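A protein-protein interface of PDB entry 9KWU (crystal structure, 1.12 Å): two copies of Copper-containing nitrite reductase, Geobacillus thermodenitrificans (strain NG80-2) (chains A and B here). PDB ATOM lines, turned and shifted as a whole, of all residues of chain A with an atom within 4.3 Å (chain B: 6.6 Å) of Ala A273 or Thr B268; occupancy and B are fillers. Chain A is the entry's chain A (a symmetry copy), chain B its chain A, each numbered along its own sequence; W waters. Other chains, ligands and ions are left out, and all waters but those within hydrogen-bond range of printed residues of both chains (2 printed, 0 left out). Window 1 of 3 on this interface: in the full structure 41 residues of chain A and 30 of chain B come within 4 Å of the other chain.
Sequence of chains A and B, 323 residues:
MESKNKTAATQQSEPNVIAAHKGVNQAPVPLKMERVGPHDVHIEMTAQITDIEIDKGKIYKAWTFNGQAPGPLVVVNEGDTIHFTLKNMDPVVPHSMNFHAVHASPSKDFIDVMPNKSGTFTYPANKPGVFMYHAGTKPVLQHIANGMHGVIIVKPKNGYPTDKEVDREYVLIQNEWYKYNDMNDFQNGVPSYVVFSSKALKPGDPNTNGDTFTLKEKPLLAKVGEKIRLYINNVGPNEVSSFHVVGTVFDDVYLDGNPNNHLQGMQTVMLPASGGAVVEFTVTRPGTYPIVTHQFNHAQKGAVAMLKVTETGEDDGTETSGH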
ATOM      1  N   ASN A 234      -4.109 -32.726  23.710  1.00  0.00           N
ATOM      2  CA  ASN A 234      -4.586 -31.957  24.853  1.00  0.00           C
ATOM      3  C   ASN A 234      -5.259 -30.703  24.313  1.00  0.00           C
ATOM      4  O   ASN A 234      -4.573 -29.758  23.931  1.00  0.00           O
ATOM      5  CB  ASN A 234      -3.411 -31.561  25.740  1.00  0.00           C
ATOM      6  CG  ASN A 234      -3.799 -30.514  26.747  1.00  0.00           C
ATOM      7  OD1 ASN A 234      -4.939 -30.522  27.235  1.00  0.00           O
ATOM      8  ND2 ASN A 234      -2.883 -29.628  27.076  1.00  0.00           N
ATOM      9  N   PRO A 237      -9.187 -26.076  27.500  1.00  0.00           N
ATOM     10  CA  PRO A 237      -8.688 -24.863  26.836  1.00  0.00           C
ATOM     11  C   PRO A 237      -7.419 -24.243  27.377  1.00  0.00           C
ATOM     12  O   PRO A 237      -6.746 -23.544  26.605  1.00  0.00           O
ATOM     13  CB  PRO A 237      -9.836 -23.852  27.029  1.00  0.00           C
ATOM     14  CG  PRO A 237     -10.598 -24.371  28.230  1.00  0.00           C
ATOM     15  CD  PRO A 237     -10.531 -25.864  28.079  1.00  0.00           C
ATOM     16  N   GLU A 239      -4.892 -25.571  30.102  1.00  0.00           N
ATOM     17  CA  GLU A 239      -3.782 -26.228  30.768  1.00  0.00           C
ATOM     18  C   GLU A 239      -2.892 -26.944  29.766  1.00  0.00           C
ATOM     19  O   GLU A 239      -3.347 -27.374  28.703  1.00  0.00           O
ATOM     20  CB  GLU A 239      -4.293 -27.258  31.774  1.00  0.00           C
ATOM     21  CG  GLU A 239      -5.246 -26.736  32.825  1.00  0.00           C
ATOM     22  CD  GLU A 239      -4.669 -25.803  33.862  1.00  0.00           C
ATOM     23  OE1 GLU A 239      -3.442 -25.713  34.023  1.00  0.00           O
ATOM     24  OE2 GLU A 239      -5.490 -25.204  34.592  1.00  0.00           O
ATOM     25  N   VAL A 240      -1.624 -27.104  30.144  1.00  0.00           N
ATOM     26  CA  VAL A 240      -0.711 -28.031  29.484  1.00  0.00           C
ATOM     27  C   VAL A 240      -0.858 -29.414  30.117  1.00  0.00           C
ATOM     28  O   VAL A 240      -1.475 -29.557  31.180  1.00  0.00           O
ATOM     29  CB  VAL A 240       0.738 -27.491  29.501  1.00  0.00           C
ATOM     30  CG1 VAL A 240       0.771 -26.105  28.871  1.00  0.00           C
ATOM     31  CG2 VAL A 240       1.310 -27.489  30.912  1.00  0.00           C
ATOM     32  N   ASP A 256       3.369 -33.813  17.626  1.00  0.00           N
ATOM     33  CA  ASP A 256       2.274 -33.404  16.748  1.00  0.00           C
ATOM     34  C   ASP A 256       1.917 -34.477  15.727  1.00  0.00           C
ATOM     35  O   ASP A 256       1.133 -34.217  14.803  1.00  0.00           O
ATOM     36  CB  ASP A 256       2.461 -32.017  16.124  1.00  0.00           C
ATOM     37  CG  ASP A 256       1.951 -30.906  17.024  1.00  0.00           C
ATOM     38  OD1 ASP A 256       1.093 -31.185  17.903  1.00  0.00           O
ATOM     39  OD2 ASP A 256       2.364 -29.741  16.816  1.00  0.00           O
ATOM     40  N   LEU A 271       2.724 -31.725  26.507  1.00  0.00           N
ATOM     41  CA  LEU A 271       1.840 -31.246  25.454  1.00  0.00           C
ATOM     42  C   LEU A 271       1.400 -29.826  25.773  1.00  0.00           C
ATOM     43  O   LEU A 271       0.790 -29.603  26.834  1.00  0.00           O
ATOM     44  CB  LEU A 271       0.601 -32.126  25.323  1.00  0.00           C
ATOM     45  CG  LEU A 271       0.830 -33.592  24.974  1.00  0.00           C
ATOM     46  CD1 LEU A 271      -0.474 -34.352  25.112  1.00  0.00           C
ATOM     47  CD2 LEU A 271       1.419 -33.766  23.571  1.00  0.00           C
ATOM     48  N   PRO A 272       1.625 -28.856  24.893  1.00  0.00           N
ATOM     49  CA  PRO A 272       1.003 -27.537  25.079  1.00  0.00           C
ATOM     50  C   PRO A 272      -0.511 -27.661  24.964  1.00  0.00           C
ATOM     51  O   PRO A 272      -1.048 -28.696  24.559  1.00  0.00           O
ATOM     52  CB  PRO A 272       1.601 -26.707  23.940  1.00  0.00           C
ATOM     53  CG  PRO A 272       1.937 -27.700  22.857  1.00  0.00           C
ATOM     54  CD  PRO A 272       2.343 -28.957  23.603  1.00  0.00           C
ATOM     55  N   ALA A 273      -1.219 -26.582  25.284  1.00  0.00           N
ATOM     56  CA  ALA A 273      -2.642 -26.517  24.944  1.00  0.00           C
ATOM     57  C   ALA A 273      -2.769 -26.537  23.423  1.00  0.00           C
ATOM     58  O   ALA A 273      -2.115 -25.736  22.745  1.00  0.00           O
ATOM     59  CB  ALA A 273      -3.264 -25.252  25.528  1.00  0.00           C
ATOM     60  N   SER A 274      -3.576 -27.473  22.900  1.00  0.00           N
ATOM     61  CA  SER A 274      -3.757 -27.872  21.497  1.00  0.00           C
ATOM     62  C   SER A 274      -2.674 -28.823  20.996  1.00  0.00           C
ATOM     63  O   SER A 274      -2.705 -29.212  19.820  1.00  0.00           O
ATOM     64  CB  SER A 274      -3.928 -26.709  20.507  1.00  0.00           C
ATOM     65  OG  SER A 274      -2.720 -26.022  20.219  1.00  0.00           O
ATOM     66  N   GLY A 275      -1.723 -29.202  21.840  1.00  0.00           N
ATOM     67  CA  GLY A 275      -0.626 -30.052  21.409  1.00  0.00           C
ATOM     68  C   GLY A 275      -1.028 -31.505  21.228  1.00  0.00           C
ATOM     69  O   GLY A 275      -1.769 -32.080  22.031  1.00  0.00           O
ATOM     70  N   SER B 241       3.878 -20.813  27.320  1.00  0.00           N
ATOM     71  CA  SER B 241       3.119 -20.360  26.157  1.00  0.00           C
ATOM     72  C   SER B 241       2.927 -21.491  25.159  1.00  0.00           C
ATOM     73  O   SER B 241       3.846 -22.271  24.898  1.00  0.00           O
ATOM     74  CB  SER B 241       3.834 -19.186  25.474  1.00  0.00           C
ATOM     75  OG  SER B 241       3.194 -18.822  24.277  1.00  0.00           O
ATOM     76  N   SER B 242       1.727 -21.562  24.590  1.00  0.00           N
ATOM     77  CA  SER B 242       1.351 -22.566  23.596  1.00  0.00           C
ATOM     78  C   SER B 242       1.179 -21.834  22.260  1.00  0.00           C
ATOM     79  O   SER B 242       0.063 -21.522  21.831  1.00  0.00           O
ATOM     80  CB  SER B 242       0.065 -23.264  24.039  1.00  0.00           C
ATOM     81  OG  SER B 242       0.277 -24.008  25.246  1.00  0.00           O
ATOM     82  N   PHE B 243       2.291 -21.533  21.594  1.00  0.00           N
ATOM     83  CA  PHE B 243       2.282 -20.555  20.508  1.00  0.00           C
ATOM     84  C   PHE B 243       1.729 -21.156  19.214  1.00  0.00           C
ATOM     85  O   PHE B 243       2.175 -22.220  18.771  1.00  0.00           O
ATOM     86  CB  PHE B 243       3.696 -20.034  20.289  1.00  0.00           C
ATOM     87  CG  PHE B 243       3.755 -18.916  19.308  1.00  0.00           C
ATOM     88  CD1 PHE B 243       3.452 -17.615  19.686  1.00  0.00           C
ATOM     89  CD2 PHE B 243       4.054 -19.159  17.970  1.00  0.00           C
ATOM     90  CE1 PHE B 243       3.481 -16.578  18.763  1.00  0.00           C
ATOM     91  CE2 PHE B 243       4.082 -18.124  17.047  1.00  0.00           C
ATOM     92  CZ  PHE B 243       3.804 -16.838  17.444  1.00  0.00           C
ATOM     93  N   HIS B 244       0.739 -20.483  18.610  1.00  0.00           N
ATOM     94  CA  HIS B 244       0.021 -21.019  17.460  1.00  0.00           C
ATOM     95  C   HIS B 244      -0.403 -19.894  16.524  1.00  0.00           C
ATOM     96  O   HIS B 244      -0.869 -18.849  16.985  1.00  0.00           O
ATOM     97  CB  HIS B 244      -1.248 -21.728  17.969  1.00  0.00           C
ATOM     98  CG  HIS B 244      -2.129 -22.266  16.887  1.00  0.00           C
ATOM     99  ND1 HIS B 244      -1.825 -23.414  16.182  1.00  0.00           N
ATOM    100  CD2 HIS B 244      -3.305 -21.818  16.381  1.00  0.00           C
ATOM    101  CE1 HIS B 244      -2.760 -23.635  15.276  1.00  0.00           C
ATOM    102  NE2 HIS B 244      -3.682 -22.695  15.390  1.00  0.00           N
ATOM    103  N   VAL B 245      -0.281 -20.119  15.211  1.00  0.00           N
ATOM    104  CA  VAL B 245      -0.825 -19.225  14.189  1.00  0.00           C
ATOM    105  C   VAL B 245      -2.030 -19.907  13.546  1.00  0.00           C
ATOM    106  O   VAL B 245      -1.927 -21.016  13.014  1.00  0.00           O
ATOM    107  CB  VAL B 245       0.229 -18.821  13.146  1.00  0.00           C
ATOM    108  CG1 VAL B 245      -0.386 -17.880  12.108  1.00  0.00           C
ATOM    109  CG2 VAL B 245       1.439 -18.157  13.810  1.00  0.00           C
ATOM    110  N   VAL B 249       0.198 -24.130   9.575  1.00  0.00           N
ATOM    111  CA  VAL B 249       0.976 -25.066  10.378  1.00  0.00           C
ATOM    112  C   VAL B 249       2.426 -24.602  10.275  1.00  0.00           C
ATOM    113  O   VAL B 249       2.838 -24.106   9.226  1.00  0.00           O
ATOM    114  CB  VAL B 249       0.824 -26.506   9.822  1.00  0.00           C
ATOM    115  CG1 VAL B 249       1.585 -27.498  10.676  1.00  0.00           C
ATOM    116  CG2 VAL B 249      -0.651 -26.905   9.699  1.00  0.00           C
ATOM    117  N   PHE B 250       3.215 -24.751  11.335  1.00  0.00           N
ATOM    118  CA  PHE B 250       4.620 -24.372  11.212  1.00  0.00           C
ATOM    119  C   PHE B 250       5.336 -25.381  10.317  1.00  0.00           C
ATOM    120  O   PHE B 250       5.427 -26.568  10.645  1.00  0.00           O
ATOM    121  CB  PHE B 250       5.282 -24.259  12.581  1.00  0.00           C
ATOM    122  CG  PHE B 250       4.653 -23.203  13.458  1.00  0.00           C
ATOM    123  CD1 PHE B 250       4.623 -21.866  13.075  1.00  0.00           C
ATOM    124  CD2 PHE B 250       4.038 -23.564  14.647  1.00  0.00           C
ATOM    125  CE1 PHE B 250       4.015 -20.918  13.862  1.00  0.00           C
ATOM    126  CE2 PHE B 250       3.422 -22.607  15.449  1.00  0.00           C
ATOM    127  CZ  PHE B 250       3.408 -21.286  15.052  1.00  0.00           C
ATOM    128  N   GLY B 265       6.425 -29.294  10.823  1.00  0.00           N
ATOM    129  CA  GLY B 265       4.997 -29.585  10.809  1.00  0.00           C
ATOM    130  C   GLY B 265       4.319 -29.521  12.157  1.00  0.00           C
ATOM    131  O   GLY B 265       3.424 -30.329  12.441  1.00  0.00           O
ATOM    132  N   MET B 266       4.734 -28.583  13.010  1.00  0.00           N
ATOM    133  CA  MET B 266       4.127 -28.406  14.326  1.00  0.00           C
ATOM    134  C   MET B 266       2.912 -27.486  14.235  1.00  0.00           C
ATOM    135  O   MET B 266       2.968 -26.430  13.602  1.00  0.00           O
ATOM    136  CB  MET B 266       5.127 -27.774  15.299  1.00  0.00           C
ATOM    137  CG  MET B 266       6.377 -28.606  15.549  1.00  0.00           C
ATOM    138  SD  MET B 266       6.112 -30.141  16.493  1.00  0.00           S
ATOM    139  CE  MET B 266       5.601 -29.498  18.089  1.00  0.00           C
ATOM    140  N   GLN B 267       1.817 -27.867  14.897  1.00  0.00           N
ATOM    141  CA  GLN B 267       0.670 -26.973  14.992  1.00  0.00           C
ATOM    142  C   GLN B 267       0.916 -25.863  16.011  1.00  0.00           C
ATOM    143  O   GLN B 267       0.493 -24.719  15.803  1.00  0.00           O
ATOM    144  CB  GLN B 267      -0.623 -27.729  15.320  1.00  0.00           C
ATOM    145  CG  GLN B 267      -0.794 -28.228  16.751  1.00  0.00           C
ATOM    146  CD  GLN B 267      -1.918 -29.236  16.817  1.00  0.00           C
ATOM    147  OE1 GLN B 267      -3.091 -28.894  16.610  1.00  0.00           O
ATOM    148  NE2 GLN B 267      -1.566 -30.497  17.069  1.00  0.00           N
ATOM    149  N   THR B 268       1.592 -26.194  17.114  1.00  0.00           N
ATOM    150  CA  THR B 268       1.722 -25.339  18.290  1.00  0.00           C
ATOM    151  C   THR B 268       3.080 -25.609  18.917  1.00  0.00           C
ATOM    152  O   THR B 268       3.502 -26.768  19.006  1.00  0.00           O
ATOM    153  CB  THR B 268       0.572 -25.639  19.266  1.00  0.00           C
ATOM    154  OG1 THR B 268      -0.637 -25.270  18.585  1.00  0.00           O
ATOM    155  CG2 THR B 268       0.712 -24.875  20.578  1.00  0.00           C
ATOM    156  N   VAL B 269       3.769 -24.546  19.337  1.00  0.00           N
ATOM    157  CA  VAL B 269       5.099 -24.661  19.930  1.00  0.00           C
ATOM    158  C   VAL B 269       5.024 -24.340  21.422  1.00  0.00           C
ATOM    159  O   VAL B 269       4.654 -23.231  21.812  1.00  0.00           O
ATOM    160  CB  VAL B 269       6.111 -23.757  19.208  1.00  0.00           C
ATOM    161  CG1 VAL B 269       7.476 -23.793  19.884  1.00  0.00           C
ATOM    162  CG2 VAL B 269       6.234 -24.170  17.746  1.00  0.00           C
ATOM    163  N   MET B 270       5.377 -25.322  22.255  1.00  0.00           N
ATOM    164  CA  MET B 270       5.502 -25.168  23.705  1.00  0.00           C
ATOM    165  C   MET B 270       6.723 -24.362  24.068  1.00  0.00           C
ATOM    166  O   MET B 270       7.846 -24.818  23.832  1.00  0.00           O
ATOM    167  CB  MET B 270       5.531 -26.565  24.325  1.00  0.00           C
ATOM    168  CG  MET B 270       5.697 -26.648  25.826  1.00  0.00           C
ATOM    169  SD  MET B 270       4.105 -26.534  26.721  1.00  0.00           S
ATOM    170  CE  MET B 270       3.841 -24.877  26.872  1.00  0.00           C
ATOM    171  N   THR B 293      -1.385 -17.368  22.023  1.00  0.00           N
ATOM    172  CA  THR B 293      -1.115 -18.514  22.888  1.00  0.00           C
ATOM    173  C   THR B 293      -2.420 -19.299  23.017  1.00  0.00           C
ATOM    174  O   THR B 293      -3.477 -18.716  23.276  1.00  0.00           O
ATOM    175  CB  THR B 293      -0.540 -18.145  24.262  1.00  0.00           C
ATOM    176  OG1 THR B 293      -0.443 -19.380  25.008  1.00  0.00           O
ATOM    177  CG2 THR B 293      -1.391 -17.139  25.011  1.00  0.00           C
ATOM    178  N   HIS B 294      -2.349 -20.617  22.813  1.00  0.00           N
ATOM    179  CA  HIS B 294      -3.545 -21.452  22.795  1.00  0.00           C
ATOM    180  C   HIS B 294      -4.015 -21.827  24.188  1.00  0.00           C
ATOM    181  O   HIS B 294      -5.008 -22.549  24.307  1.00  0.00           O
ATOM    182  CB  HIS B 294      -3.347 -22.707  21.933  1.00  0.00           C
ATOM    183  CG  HIS B 294      -4.535 -23.037  21.074  1.00  0.00           C
ATOM    184  ND1 HIS B 294      -5.686 -23.621  21.553  1.00  0.00           N
ATOM    185  CD2 HIS B 294      -4.759 -22.799  19.760  1.00  0.00           C
ATOM    186  CE1 HIS B 294      -6.560 -23.736  20.565  1.00  0.00           C
ATOM    187  NE2 HIS B 294      -6.017 -23.261  19.459  1.00  0.00           N
ATOM    188  N   GLN B 295      -3.321 -21.362  25.232  1.00  0.00           N
ATOM    189  CA  GLN B 295      -3.865 -21.323  26.593  1.00  0.00           C
ATOM    190  C   GLN B 295      -4.875 -20.196  26.575  1.00  0.00           C
ATOM    191  O   GLN B 295      -4.512 -19.023  26.664  1.00  0.00           O
ATOM    192  CB  GLN B 295      -2.738 -21.140  27.602  1.00  0.00           C
ATOM    193  CG  GLN B 295      -1.836 -22.375  27.640  1.00  0.00           C
ATOM    194  CD  GLN B 295      -0.421 -22.089  28.118  1.00  0.00           C
ATOM    195  OE1 GLN B 295       0.551 -22.386  27.420  1.00  0.00           O
ATOM    196  NE2 GLN B 295      -0.294 -21.562  29.328  1.00  0.00           N
ATOM    197  N   PHE B 296      -6.150 -20.542  26.351  1.00  0.00           N
ATOM    198  CA  PHE B 296      -7.105 -19.536  25.888  1.00  0.00           C
ATOM    199  C   PHE B 296      -7.540 -18.571  26.980  1.00  0.00           C
ATOM    200  O   PHE B 296      -8.053 -17.493  26.645  1.00  0.00           O
ATOM    201  CB  PHE B 296      -8.280 -20.137  25.085  1.00  0.00           C
ATOM    202  CG  PHE B 296      -8.155 -19.835  23.616  1.00  0.00           C
ATOM    203  CD1 PHE B 296      -8.561 -18.604  23.125  1.00  0.00           C
ATOM    204  CD2 PHE B 296      -7.494 -20.704  22.762  1.00  0.00           C
ATOM    205  CE1 PHE B 296      -8.341 -18.264  21.807  1.00  0.00           C
ATOM    206  CE2 PHE B 296      -7.277 -20.367  21.428  1.00  0.00           C
ATOM    207  CZ  PHE B 296      -7.694 -19.134  20.954  1.00  0.00           C
HETATM  208  O   HOH W   1      -6.866 -24.696  23.824  1.00  0.00           O
HETATM  209  O   HOH W   2       2.043 -29.086  19.698  1.00  0.00           O
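No position is printed for both chains.
Of the 18 pairs that touch across the chains among the printed residues, none has its exchanged pair printed and touching as well.
Among the printed residues, merely in contact across the chains: Pro A237 with Gln B295 (3.6 Å), Val A240 with Met B270 (3.9 Å), Val A240 with Gln B295 (3.998 Å), Asp A256 with Thr B268 (3.6 Å), Pro A272 with Ser B242 (3.3 Å), Pro A272 with Thr B268 (3.8 Å), Pro A272 with Met B270 (3.7 Å), Ala A273 with Thr B268 (3.7 Å), Ala A273 with His B294 (3.4 Å), Ala A273 with Gln B295 (3.8 Å) and Ser A274 with His B294 (3.6 Å).
Hydrophobic or aromatic side chains of chain B that line the printed part of chain A: Met B266, Met B270 and His B294.
Among the printed residues, 18 pairs touch across the chains.
Among the printed residues, no Asp or Glu carboxylate lies within 4 Å of a Lys or Arg side-chain nitrogen of the other chain.
Ala A273 touches four residues of chain B.
Ser B241 touches none of the printed residues of chain A.
Of the printed residues of chain A, Ser B242 touches Pro A272 (3.3 Å) and Ala A273 (3.0 Å).
Of the printed residues of chain A, Phe B296 touches Pro A237.
The nearest residue of chain B that does not touch Ala A273 is Met B270 (5.5 Å).
The nearest printed residue of chain A that does not touch Thr B268 is Gly A275 (5.0 Å).
The nearest printed residue of chain A that does not touch Met B266 is Pro A272 (6.3 Å).
The side-chain amide nitrogen of Asn A234 sits at hydrogen-bond distance from the backbone carbonyl oxygen of Pro A272, at 3.3 Å.
The backbone NH (N) of Ser A274 sits at hydrogen-bond distance from the backbone carbonyl oxygen (O) of Asn A234.
N of Ser B242 sits at hydrogen-bond distance from OG1 of Thr B293, 3.1 Å away.
The backbone carbonyl oxygen (O) of Ser B242 is in hydrogen-bond range of the backbone NH (N) of His B294 (2.8 Å).
OG of Ser B242 is in hydrogen-bond range of OE1 of Gln B295.
The backbone NH of Phe B250 sits at hydrogen-bond distance from the backbone carbonyl oxygen of Met B266 (2.8 Å).
OG1 of Thr B268 is in hydrogen-bond range of OG of Ser A274 (2.8 Å).
O of Pro A237 sits close to O of His B294, at 3.0 Å.
OG of Ser B242 is in hydrogen-bond range of N of Ala A273, 3.0 Å away.
N of Gln B267 sits at hydrogen-bond distance from OD2 of Asp A256.
N of Phe B296 sits at hydrogen-bond distance from O of Pro A237, 3.1 Å away.
The side-chain amide nitrogen (NE2) of Gln B267 sits close to the backbone carbonyl oxygen (O) of Ser A274, at 3.2 Å.
SD of Met B266 sits close to OD2 of Asp A256, at 3.8 Å.
Water W1 bridges a ring nitrogen (ND1) of His B294 (2.8 Å) and the backbone carbonyl oxygen of Pro A237 (3.0 Å).
Water W2 lies within hydrogen-bond range of the backbone carbonyl oxygen (O) of Thr B268 (2.8 Å) and the side-chain carboxylate (OD1) of Asp A256 (2.9 Å).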
